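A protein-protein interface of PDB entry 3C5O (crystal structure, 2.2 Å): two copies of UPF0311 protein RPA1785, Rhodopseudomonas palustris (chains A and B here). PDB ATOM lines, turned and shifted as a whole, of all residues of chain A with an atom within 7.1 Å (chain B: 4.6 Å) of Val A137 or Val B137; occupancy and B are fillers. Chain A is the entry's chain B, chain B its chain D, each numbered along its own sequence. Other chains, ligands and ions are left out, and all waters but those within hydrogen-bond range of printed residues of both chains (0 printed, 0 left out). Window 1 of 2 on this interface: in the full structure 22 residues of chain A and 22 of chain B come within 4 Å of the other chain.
The guanidinium group (NH1) of Arg A116 sits at hydrogen-bond distance from the side-chain hydroxyl (OG) of Ser A139 (3.4 Å).
The backbone carbonyl oxygen (O) of Leu A135 sits at hydrogen-bond distance from the backbone NH (N) of Val A154, 2.8 Å away.
O of Asp B150 sits at hydrogen-bond distance from N of Ser B139.
The backbone NH (N) of Gly A138 is in hydrogen-bond range of the backbone carbonyl oxygen (O) of Thr A117.
The side-chain amide oxygen (OD1) of Asn A88 lies within hydrogen-bond range of the side-chain hydroxyl (OG1) of Thr A117 (2.6 Å).
The backbone NH (N) of His A152 lies within hydrogen-bond range of the backbone carbonyl oxygen (O) of Val A137, at 2.8 Å.
Val B137 touches Leu A7 (CG1 to CD2, 3.8 Å).
N of Leu A7 touches CE1 of His B152 (3.7 Å).
CG2 of Thr A9 touches CD2 of Leu B7, at 3.96 Å.
Leu B135 touches Arg A116.
Arg A116 touches Val B154 (CD to CG1, 3.8 Å).
Thr A117 touches Leu B135.
Arg A118 touches Leu B135.
Leu A135 touches Val B137.
Val A137 touches Leu B7.
Val A137 touches Val B137 (CG2 to CG2, 3.6 Å).
Of the printed residues of chain B, Thr A117 touches Leu B135 (3.4 Å).
Of the printed residues of chain B, Arg A118 touches Leu B135 (3.98 Å).
Printed residues of chain B within 4 Å of Leu A135: Thr B117 and Val B137.
Of the printed residues of chain B, Val A137 touches Leu B7 and Val B137.
Printed residues of chain A within 4 Å of Leu B135: Arg A116, Thr A117 and Arg A118.
Of the printed residues of chain A, Val B137 touches Leu A7, Leu A135 and Val A137.
Printed residues of chain A within 4 Å of Ser B139: Leu A7 (3.7 Å).
The nearest printed residue of chain B that does not touch Val A137 is Val B154 (4.2 Å).
The nearest residue of chain A that does not touch Val B137 is Val A154 (4.3 Å).
Hydrophobic or aromatic side chains of chain B within 4 Å of the printed part of chain A: Leu B7, Leu B135, Val B137, His B152 and Val B154.
Of the 21 printed residues of chain A, 8 touch a printed residue of chain B.
Hydrophobic or aromatic side chains of chain A that line the printed part of chain B: Leu A7, Leu A135, Val A137 and His A152.
Leu A7 touches Val B137, and with the chains exchanged Val A137 touches Leu B7.
Thr A117 touches Leu B135, and with the chains exchanged Leu A135 touches Thr B117.
Leu A135 touches Val B137, but with the chains exchanged Val A137 does not touch Leu B135 (4.3 Å).
Val A137 touches its own counterpart, Val B137.
Positions printed for both chains: 7, 117, 119, 135, 136, 137, 138, 139, 150, 151, 152 and 154.
Of the 13 pairs that touch across the chains among the printed residues, 7 have their exchanged pair printed and touching as well.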
ATOM      1  N   LEU A   7      26.753  -4.789   5.748  1.00  0.00           N
ATOM      2  CA  LEU A   7      27.561  -5.977   5.482  1.00  0.00           C
ATOM      3  C   LEU A   7      28.554  -5.624   4.397  1.00  0.00           C
ATOM      4  O   LEU A   7      28.174  -5.082   3.362  1.00  0.00           O
ATOM      5  CB  LEU A   7      26.685  -7.153   5.020  1.00  0.00           C
ATOM      6  CG  LEU A   7      27.320  -8.545   5.042  1.00  0.00           C
ATOM      7  CD1 LEU A   7      27.451  -9.047   6.464  1.00  0.00           C
ATOM      8  CD2 LEU A   7      26.541  -9.550   4.169  1.00  0.00           C
ATOM      9  N   THR A   9      31.532  -7.099   1.831  1.00  0.00           N
ATOM     10  CA  THR A   9      32.139  -8.248   1.182  1.00  0.00           C
ATOM     11  C   THR A   9      33.245  -7.752   0.274  1.00  0.00           C
ATOM     12  O   THR A   9      33.342  -6.564   0.016  1.00  0.00           O
ATOM     13  CB  THR A   9      31.131  -9.093   0.345  1.00  0.00           C
ATOM     14  OG1 THR A   9      30.691  -8.344  -0.794  1.00  0.00           O
ATOM     15  CG2 THR A   9      29.951  -9.520   1.183  1.00  0.00           C
ATOM     16  N   LYS A  10      34.078  -8.672  -0.194  1.00  0.00           N
ATOM     17  CA  LYS A  10      35.169  -8.364  -1.105  1.00  0.00           C
ATOM     18  C   LYS A  10      35.356  -9.568  -2.032  1.00  0.00           C
ATOM     19  O   LYS A  10      35.494 -10.697  -1.570  1.00  0.00           O
ATOM     20  CB  LYS A  10      36.446  -8.068  -0.302  1.00  0.00           C
ATOM     21  CG  LYS A  10      37.752  -8.270  -1.046  1.00  0.00           C
ATOM     22  CD  LYS A  10      38.947  -8.199  -0.099  1.00  0.00           C
ATOM     23  CE  LYS A  10      40.163  -8.888  -0.688  1.00  0.00           C
ATOM     24  NZ  LYS A  10      41.073  -9.320   0.422  1.00  0.00           N
ATOM     25  N   VAL A  12      37.139 -12.229  -4.051  1.00  0.00           N
ATOM     26  CA  VAL A  12      38.464 -12.812  -3.876  1.00  0.00           C
ATOM     27  C   VAL A  12      38.910 -13.688  -5.055  1.00  0.00           C
ATOM     28  O   VAL A  12      40.046 -13.594  -5.486  1.00  0.00           O
ATOM     29  CB  VAL A  12      38.638 -13.576  -2.514  1.00  0.00           C
ATOM     30  CG1 VAL A  12      38.739 -12.600  -1.362  1.00  0.00           C
ATOM     31  CG2 VAL A  12      37.502 -14.574  -2.281  1.00  0.00           C
ATOM     32  N   PHE A  13      38.051 -14.560  -5.564  1.00  0.00           N
ATOM     33  CA  PHE A  13      38.482 -15.389  -6.697  1.00  0.00           C
ATOM     34  C   PHE A  13      37.327 -16.023  -7.400  1.00  0.00           C
ATOM     35  O   PHE A  13      36.214 -16.030  -6.877  1.00  0.00           O
ATOM     36  CB  PHE A  13      39.530 -16.462  -6.279  1.00  0.00           C
ATOM     37  CG  PHE A  13      39.112 -17.330  -5.114  1.00  0.00           C
ATOM     38  CD1 PHE A  13      39.567 -17.047  -3.825  1.00  0.00           C
ATOM     39  CD2 PHE A  13      38.291 -18.439  -5.306  1.00  0.00           C
ATOM     40  CE1 PHE A  13      39.192 -17.830  -2.762  1.00  0.00           C
ATOM     41  CE2 PHE A  13      37.913 -19.242  -4.231  1.00  0.00           C
ATOM     42  CZ  PHE A  13      38.367 -18.936  -2.959  1.00  0.00           C
ATOM     43  N   ASN A  88      30.057 -26.669  -1.843  1.00  0.00           N
ATOM     44  CA  ASN A  88      29.359 -25.483  -2.374  1.00  0.00           C
ATOM     45  C   ASN A  88      27.818 -25.659  -2.363  1.00  0.00           C
ATOM     46  O   ASN A  88      27.256 -26.437  -3.151  1.00  0.00           O
ATOM     47  CB  ASN A  88      29.881 -25.204  -3.780  1.00  0.00           C
ATOM     48  CG  ASN A  88      29.553 -23.805  -4.292  1.00  0.00           C
ATOM     49  OD1 ASN A  88      29.341 -22.860  -3.531  1.00  0.00           O
ATOM     50  ND2 ASN A  88      29.527 -23.679  -5.623  1.00  0.00           N
ATOM     51  N   ARG A 116      23.118 -18.182  -6.322  1.00  0.00           N
ATOM     52  CA  ARG A 116      23.944 -17.808  -5.189  1.00  0.00           C
ATOM     53  C   ARG A 116      24.161 -19.003  -4.278  1.00  0.00           C
ATOM     54  O   ARG A 116      23.255 -19.841  -4.079  1.00  0.00           O
ATOM     55  CB  ARG A 116      23.352 -16.624  -4.399  1.00  0.00           C
ATOM     56  CG  ARG A 116      22.801 -15.439  -5.269  1.00  0.00           C
ATOM     57  CD  ARG A 116      23.860 -14.449  -5.824  1.00  0.00           C
ATOM     58  NE  ARG A 116      23.192 -13.364  -6.576  1.00  0.00           N
ATOM     59  CZ  ARG A 116      22.881 -13.415  -7.874  1.00  0.00           C
ATOM     60  NH1 ARG A 116      23.209 -14.460  -8.593  1.00  0.00           N
ATOM     61  NH2 ARG A 116      22.273 -12.403  -8.482  1.00  0.00           N
ATOM     62  N   THR A 117      25.371 -19.077  -3.729  1.00  0.00           N
ATOM     63  CA  THR A 117      25.779 -20.212  -2.940  1.00  0.00           C
ATOM     64  C   THR A 117      26.639 -19.774  -1.767  1.00  0.00           C
ATOM     65  O   THR A 117      27.097 -18.625  -1.697  1.00  0.00           O
ATOM     66  CB  THR A 117      26.665 -21.183  -3.759  1.00  0.00           C
ATOM     67  OG1 THR A 117      27.978 -20.626  -3.859  1.00  0.00           O
ATOM     68  CG2 THR A 117      26.138 -21.413  -5.149  1.00  0.00           C
ATOM     69  N   ARG A 118      26.874 -20.708  -0.850  1.00  0.00           N
ATOM     70  CA  ARG A 118      27.855 -20.482   0.212  1.00  0.00           C
ATOM     71  C   ARG A 118      28.935 -21.540   0.060  1.00  0.00           C
ATOM     72  O   ARG A 118      28.701 -22.689   0.392  1.00  0.00           O
ATOM     73  CB  ARG A 118      27.224 -20.579   1.588  1.00  0.00           C
ATOM     74  CG  ARG A 118      28.210 -20.206   2.665  1.00  0.00           C
ATOM     75  CD  ARG A 118      28.070 -21.072   3.886  1.00  0.00           C
ATOM     76  NE  ARG A 118      29.348 -21.134   4.583  1.00  0.00           N
ATOM     77  CZ  ARG A 118      29.528 -21.674   5.780  1.00  0.00           C
ATOM     78  NH1 ARG A 118      28.499 -22.178   6.454  1.00  0.00           N
ATOM     79  NH2 ARG A 118      30.738 -21.673   6.316  1.00  0.00           N
ATOM     80  N   PRO A 119      30.104 -21.160  -0.486  1.00  0.00           N
ATOM     81  CA  PRO A 119      31.234 -22.083  -0.520  1.00  0.00           C
ATOM     82  C   PRO A 119      32.023 -22.178   0.786  1.00  0.00           C
ATOM     83  O   PRO A 119      32.436 -21.146   1.359  1.00  0.00           O
ATOM     84  CB  PRO A 119      32.098 -21.543  -1.650  1.00  0.00           C
ATOM     85  CG  PRO A 119      31.747 -20.068  -1.736  1.00  0.00           C
ATOM     86  CD  PRO A 119      30.399 -19.872  -1.137  1.00  0.00           C
ATOM     87  N   LEU A 135      33.502 -16.566   6.285  1.00  0.00           N
ATOM     88  CA  LEU A 135      32.396 -17.049   5.478  1.00  0.00           C
ATOM     89  C   LEU A 135      32.571 -16.500   4.070  1.00  0.00           C
ATOM     90  O   LEU A 135      33.123 -15.401   3.885  1.00  0.00           O
ATOM     91  CB  LEU A 135      31.093 -16.535   6.057  1.00  0.00           C
ATOM     92  CG  LEU A 135      29.758 -17.208   5.811  1.00  0.00           C
ATOM     93  CD1 LEU A 135      29.640 -18.340   6.769  1.00  0.00           C
ATOM     94  CD2 LEU A 135      28.662 -16.199   6.077  1.00  0.00           C
ATOM     95  N   PHE A 136      32.091 -17.241   3.076  1.00  0.00           N
ATOM     96  CA  PHE A 136      32.178 -16.786   1.700  1.00  0.00           C
ATOM     97  C   PHE A 136      30.818 -16.923   1.055  1.00  0.00           C
ATOM     98  O   PHE A 136      30.001 -17.773   1.446  1.00  0.00           O
ATOM     99  CB  PHE A 136      33.213 -17.589   0.906  1.00  0.00           C
ATOM    100  CG  PHE A 136      34.616 -17.486   1.438  1.00  0.00           C
ATOM    101  CD1 PHE A 136      35.528 -16.612   0.871  1.00  0.00           C
ATOM    102  CD2 PHE A 136      35.045 -18.306   2.481  1.00  0.00           C
ATOM    103  CE1 PHE A 136      36.838 -16.511   1.366  1.00  0.00           C
ATOM    104  CE2 PHE A 136      36.349 -18.221   2.972  1.00  0.00           C
ATOM    105  CZ  PHE A 136      37.249 -17.318   2.413  1.00  0.00           C
ATOM    106  N   VAL A 137      30.557 -16.072   0.071  1.00  0.00           N
ATOM    107  CA  VAL A 137      29.325 -16.181  -0.714  1.00  0.00           C
ATOM    108  C   VAL A 137      29.723 -16.272  -2.182  1.00  0.00           C
ATOM    109  O   VAL A 137      30.592 -15.552  -2.640  1.00  0.00           O
ATOM    110  CB  VAL A 137      28.394 -14.969  -0.484  1.00  0.00           C
ATOM    111  CG1 VAL A 137      27.124 -15.065  -1.335  1.00  0.00           C
ATOM    112  CG2 VAL A 137      28.002 -14.873   0.973  1.00  0.00           C
ATOM    113  N   GLY A 138      29.089 -17.169  -2.923  1.00  0.00           N
ATOM    114  CA  GLY A 138      29.342 -17.274  -4.356  1.00  0.00           C
ATOM    115  C   GLY A 138      28.203 -16.742  -5.200  1.00  0.00           C
ATOM    116  O   GLY A 138      27.052 -17.038  -4.923  1.00  0.00           O
ATOM    117  N   SER A 139      28.515 -15.961  -6.226  1.00  0.00           N
ATOM    118  CA  SER A 139      27.508 -15.562  -7.213  1.00  0.00           C
ATOM    119  C   SER A 139      27.923 -16.283  -8.483  1.00  0.00           C
ATOM    120  O   SER A 139      29.075 -16.126  -8.941  1.00  0.00           O
ATOM    121  CB  SER A 139      27.496 -14.054  -7.416  1.00  0.00           C
ATOM    122  OG  SER A 139      26.508 -13.661  -8.353  1.00  0.00           O
ATOM    123  N   ILE A 149      31.705 -19.543 -10.653  1.00  0.00           N
ATOM    124  CA  ILE A 149      31.328 -19.016  -9.347  1.00  0.00           C
ATOM    125  C   ILE A 149      32.304 -17.925  -9.004  1.00  0.00           C
ATOM    126  O   ILE A 149      33.494 -18.186  -8.855  1.00  0.00           O
ATOM    127  CB  ILE A 149      31.525 -20.035  -8.168  1.00  0.00           C
ATOM    128  CG1 ILE A 149      31.514 -21.537  -8.594  1.00  0.00           C
ATOM    129  CG2 ILE A 149      30.685 -19.623  -6.917  1.00  0.00           C
ATOM    130  CD1 ILE A 149      30.241 -22.123  -8.889  1.00  0.00           C
ATOM    131  N   ASP A 150      31.798 -16.718  -8.836  1.00  0.00           N
ATOM    132  CA  ASP A 150      32.591 -15.616  -8.336  1.00  0.00           C
ATOM    133  C   ASP A 150      32.462 -15.620  -6.837  1.00  0.00           C
ATOM    134  O   ASP A 150      31.364 -15.436  -6.304  1.00  0.00           O
ATOM    135  CB  ASP A 150      32.079 -14.307  -8.908  1.00  0.00           C
ATOM    136  CG  ASP A 150      32.289 -14.222 -10.391  1.00  0.00           C
ATOM    137  OD1 ASP A 150      33.427 -14.463 -10.851  1.00  0.00           O
ATOM    138  OD2 ASP A 150      31.315 -13.908 -11.104  1.00  0.00           O
ATOM    139  N   VAL A 151      33.582 -15.835  -6.165  1.00  0.00           N
ATOM    140  CA  VAL A 151      33.607 -16.051  -4.715  1.00  0.00           C
ATOM    141  C   VAL A 151      33.947 -14.738  -4.007  1.00  0.00           C
ATOM    142  O   VAL A 151      34.917 -14.067  -4.346  1.00  0.00           O
ATOM    143  CB  VAL A 151      34.623 -17.179  -4.307  1.00  0.00           C
ATOM    144  CG1 VAL A 151      34.651 -17.385  -2.787  1.00  0.00           C
ATOM    145  CG2 VAL A 151      34.289 -18.524  -5.006  1.00  0.00           C
ATOM    146  N   HIS A 152      33.136 -14.389  -3.018  1.00  0.00           N
ATOM    147  CA  HIS A 152      33.310 -13.175  -2.269  1.00  0.00           C
ATOM    148  C   HIS A 152      33.540 -13.511  -0.814  1.00  0.00           C
ATOM    149  O   HIS A 152      32.811 -14.315  -0.250  1.00  0.00           O
ATOM    150  CB  HIS A 152      32.063 -12.310  -2.413  1.00  0.00           C
ATOM    151  CG  HIS A 152      31.729 -11.999  -3.834  1.00  0.00           C
ATOM    152  ND1 HIS A 152      32.183 -10.871  -4.469  1.00  0.00           N
ATOM    153  CD2 HIS A 152      31.023 -12.691  -4.758  1.00  0.00           C
ATOM    154  CE1 HIS A 152      31.750 -10.858  -5.715  1.00  0.00           C
ATOM    155  NE2 HIS A 152      31.048 -11.954  -5.920  1.00  0.00           N
ATOM    156  N   GLN A 153      34.547 -12.890  -0.216  1.00  0.00           N
ATOM    157  CA  GLN A 153      34.850 -13.050   1.195  1.00  0.00           C
ATOM    158  C   GLN A 153      33.907 -12.161   1.992  1.00  0.00           C
ATOM    159  O   GLN A 153      33.807 -10.965   1.693  1.00  0.00           O
ATOM    160  CB  GLN A 153      36.287 -12.605   1.436  1.00  0.00           C
ATOM    161  CG  GLN A 153      36.821 -12.908   2.806  1.00  0.00           C
ATOM    162  CD  GLN A 153      38.178 -12.268   3.065  1.00  0.00           C
ATOM    163  OE1 GLN A 153      38.907 -12.673   3.974  1.00  0.00           O
ATOM    164  NE2 GLN A 153      38.511 -11.249   2.288  1.00  0.00           N
ATOM    165  N   VAL A 154      33.210 -12.726   2.986  1.00  0.00           N
ATOM    166  CA  VAL A 154      32.370 -11.908   3.871  1.00  0.00           C
ATOM    167  C   VAL A 154      33.221 -11.307   4.977  1.00  0.00           C
ATOM    168  O   VAL A 154      33.874 -12.020   5.762  1.00  0.00           O
ATOM    169  CB  VAL A 154      31.195 -12.665   4.507  1.00  0.00           C
ATOM    170  CG1 VAL A 154      30.463 -11.763   5.531  1.00  0.00           C
ATOM    171  CG2 VAL A 154      30.222 -13.168   3.436  1.00  0.00           C
ATOM    172  N   LEU B   7      28.895  -8.060  -5.548  1.00  0.00           N
ATOM    173  CA  LEU B   7      27.845  -8.740  -4.804  1.00  0.00           C
ATOM    174  C   LEU B   7      26.983  -7.727  -4.078  1.00  0.00           C
ATOM    175  O   LEU B   7      27.485  -6.888  -3.310  1.00  0.00           O
ATOM    176  CB  LEU B   7      28.424  -9.734  -3.794  1.00  0.00           C
ATOM    177  CG  LEU B   7      27.423 -10.686  -3.133  1.00  0.00           C
ATOM    178  CD1 LEU B   7      27.022 -11.842  -4.083  1.00  0.00           C
ATOM    179  CD2 LEU B   7      27.983 -11.224  -1.795  1.00  0.00           C
ATOM    180  N   THR B 117      27.271 -15.652   9.855  1.00  0.00           N
ATOM    181  CA  THR B 117      26.538 -16.905   9.735  1.00  0.00           C
ATOM    182  C   THR B 117      25.803 -16.965   8.385  1.00  0.00           C
ATOM    183  O   THR B 117      25.773 -15.990   7.619  1.00  0.00           O
ATOM    184  CB  THR B 117      25.490 -17.058  10.840  1.00  0.00           C
ATOM    185  OG1 THR B 117      24.331 -16.300  10.483  1.00  0.00           O
ATOM    186  CG2 THR B 117      26.015 -16.591  12.265  1.00  0.00           C
ATOM    187  N   PRO B 119      21.980 -18.101   7.757  1.00  0.00           N
ATOM    188  CA  PRO B 119      20.712 -18.622   8.251  1.00  0.00           C
ATOM    189  C   PRO B 119      19.832 -18.992   7.096  1.00  0.00           C
ATOM    190  O   PRO B 119      19.727 -18.242   6.111  1.00  0.00           O
ATOM    191  CB  PRO B 119      20.103 -17.427   9.018  1.00  0.00           C
ATOM    192  CG  PRO B 119      20.656 -16.243   8.310  1.00  0.00           C
ATOM    193  CD  PRO B 119      21.952 -16.625   7.658  1.00  0.00           C
ATOM    194  N   LEU B 135      19.403 -16.523  -0.732  1.00  0.00           N
ATOM    195  CA  LEU B 135      20.440 -16.851   0.229  1.00  0.00           C
ATOM    196  C   LEU B 135      20.553 -15.684   1.193  1.00  0.00           C
ATOM    197  O   LEU B 135      20.347 -14.522   0.811  1.00  0.00           O
ATOM    198  CB  LEU B 135      21.775 -17.049  -0.471  1.00  0.00           C
ATOM    199  CG  LEU B 135      22.649 -18.150   0.120  1.00  0.00           C
ATOM    200  CD1 LEU B 135      22.204 -19.506  -0.453  1.00  0.00           C
ATOM    201  CD2 LEU B 135      24.124 -17.901  -0.190  1.00  0.00           C
ATOM    202  N   PHE B 136      20.870 -15.988   2.444  1.00  0.00           N
ATOM    203  CA  PHE B 136      20.961 -14.936   3.481  1.00  0.00           C
ATOM    204  C   PHE B 136      22.280 -15.050   4.233  1.00  0.00           C
ATOM    205  O   PHE B 136      22.816 -16.154   4.375  1.00  0.00           O
ATOM    206  CB  PHE B 136      19.804 -15.044   4.455  1.00  0.00           C
ATOM    207  CG  PHE B 136      18.450 -14.789   3.842  1.00  0.00           C
ATOM    208  CD1 PHE B 136      17.802 -13.575   4.048  1.00  0.00           C
ATOM    209  CD2 PHE B 136      17.809 -15.773   3.098  1.00  0.00           C
ATOM    210  CE1 PHE B 136      16.561 -13.343   3.496  1.00  0.00           C
ATOM    211  CE2 PHE B 136      16.554 -15.540   2.544  1.00  0.00           C
ATOM    212  CZ  PHE B 136      15.932 -14.316   2.751  1.00  0.00           C
ATOM    213  N   VAL B 137      22.798 -13.909   4.695  1.00  0.00           N
ATOM    214  CA  VAL B 137      23.995 -13.852   5.514  1.00  0.00           C
ATOM    215  C   VAL B 137      23.704 -13.121   6.822  1.00  0.00           C
ATOM    216  O   VAL B 137      23.179 -11.989   6.844  1.00  0.00           O
ATOM    217  CB  VAL B 137      25.166 -13.179   4.774  1.00  0.00           C
ATOM    218  CG1 VAL B 137      26.365 -13.031   5.699  1.00  0.00           C
ATOM    219  CG2 VAL B 137      25.572 -14.002   3.544  1.00  0.00           C
ATOM    220  N   GLY B 138      24.060 -13.762   7.927  1.00  0.00           N
ATOM    221  CA  GLY B 138      23.926 -13.096   9.208  1.00  0.00           C
ATOM    222  C   GLY B 138      25.267 -12.504   9.549  1.00  0.00           C
ATOM    223  O   GLY B 138      26.300 -13.135   9.320  1.00  0.00           O
ATOM    224  N   SER B 139      25.245 -11.275  10.061  1.00  0.00           N
ATOM    225  CA  SER B 139      26.399 -10.716  10.702  1.00  0.00           C
ATOM    226  C   SER B 139      25.977 -10.597  12.149  1.00  0.00           C
ATOM    227  O   SER B 139      25.005  -9.910  12.482  1.00  0.00           O
ATOM    228  CB  SER B 139      26.796  -9.374  10.114  1.00  0.00           C
ATOM    229  OG  SER B 139      27.993  -8.928  10.733  1.00  0.00           O
ATOM    230  N   ASP B 150      21.928  -9.910  12.586  1.00  0.00           N
ATOM    231  CA  ASP B 150      21.552  -9.059  11.437  1.00  0.00           C
ATOM    232  C   ASP B 150      21.473  -9.845  10.163  1.00  0.00           C
ATOM    233  O   ASP B 150      22.494 -10.214   9.572  1.00  0.00           O
ATOM    234  CB  ASP B 150      22.606  -7.998  11.187  1.00  0.00           C
ATOM    235  CG  ASP B 150      22.741  -7.037  12.344  1.00  0.00           C
ATOM    236  OD1 ASP B 150      21.708  -6.731  12.963  1.00  0.00           O
ATOM    237  OD2 ASP B 150      23.879  -6.581  12.605  1.00  0.00           O
ATOM    238  N   VAL B 151      20.255 -10.050   9.700  1.00  0.00           N
ATOM    239  CA  VAL B 151      20.048 -10.848   8.522  1.00  0.00           C
ATOM    240  C   VAL B 151      20.032  -9.931   7.297  1.00  0.00           C
ATOM    241  O   VAL B 151      19.357  -8.870   7.283  1.00  0.00           O
ATOM    242  CB  VAL B 151      18.802 -11.723   8.665  1.00  0.00           C
ATOM    243  CG1 VAL B 151      18.873 -12.854   7.676  1.00  0.00           C
ATOM    244  CG2 VAL B 151      18.751 -12.287  10.094  1.00  0.00           C
ATOM    245  N   HIS B 152      20.849 -10.324   6.321  1.00  0.00           N
ATOM    246  CA  HIS B 152      21.007  -9.620   5.069  1.00  0.00           C
ATOM    247  C   HIS B 152      20.658 -10.605   3.957  1.00  0.00           C
ATOM    248  O   HIS B 152      21.146 -11.740   3.962  1.00  0.00           O
ATOM    249  CB  HIS B 152      22.460  -9.197   4.883  1.00  0.00           C
ATOM    250  CG  HIS B 152      22.930  -8.165   5.858  1.00  0.00           C
ATOM    251  ND1 HIS B 152      22.944  -6.823   5.562  1.00  0.00           N
ATOM    252  CD2 HIS B 152      23.410  -8.278   7.118  1.00  0.00           C
ATOM    253  CE1 HIS B 152      23.396  -6.148   6.603  1.00  0.00           C
ATOM    254  NE2 HIS B 152      23.687  -7.010   7.560  1.00  0.00           N
ATOM    255  N   VAL B 154      20.905 -11.774   0.132  1.00  0.00           N
ATOM    256  CA  VAL B 154      21.830 -11.727  -0.993  1.00  0.00           C
ATOM    257  C   VAL B 154      21.003 -11.597  -2.277  1.00  0.00           C
ATOM    258  O   VAL B 154      20.036 -12.333  -2.508  1.00  0.00           O
ATOM    259  CB  VAL B 154      22.713 -13.007  -1.098  1.00  0.00           C
ATOM    260  CG1 VAL B 154      23.683 -12.933  -2.304  1.00  0.00           C
ATOM    261  CG2 VAL B 154      23.470 -13.317   0.219  1.00  0.00           C
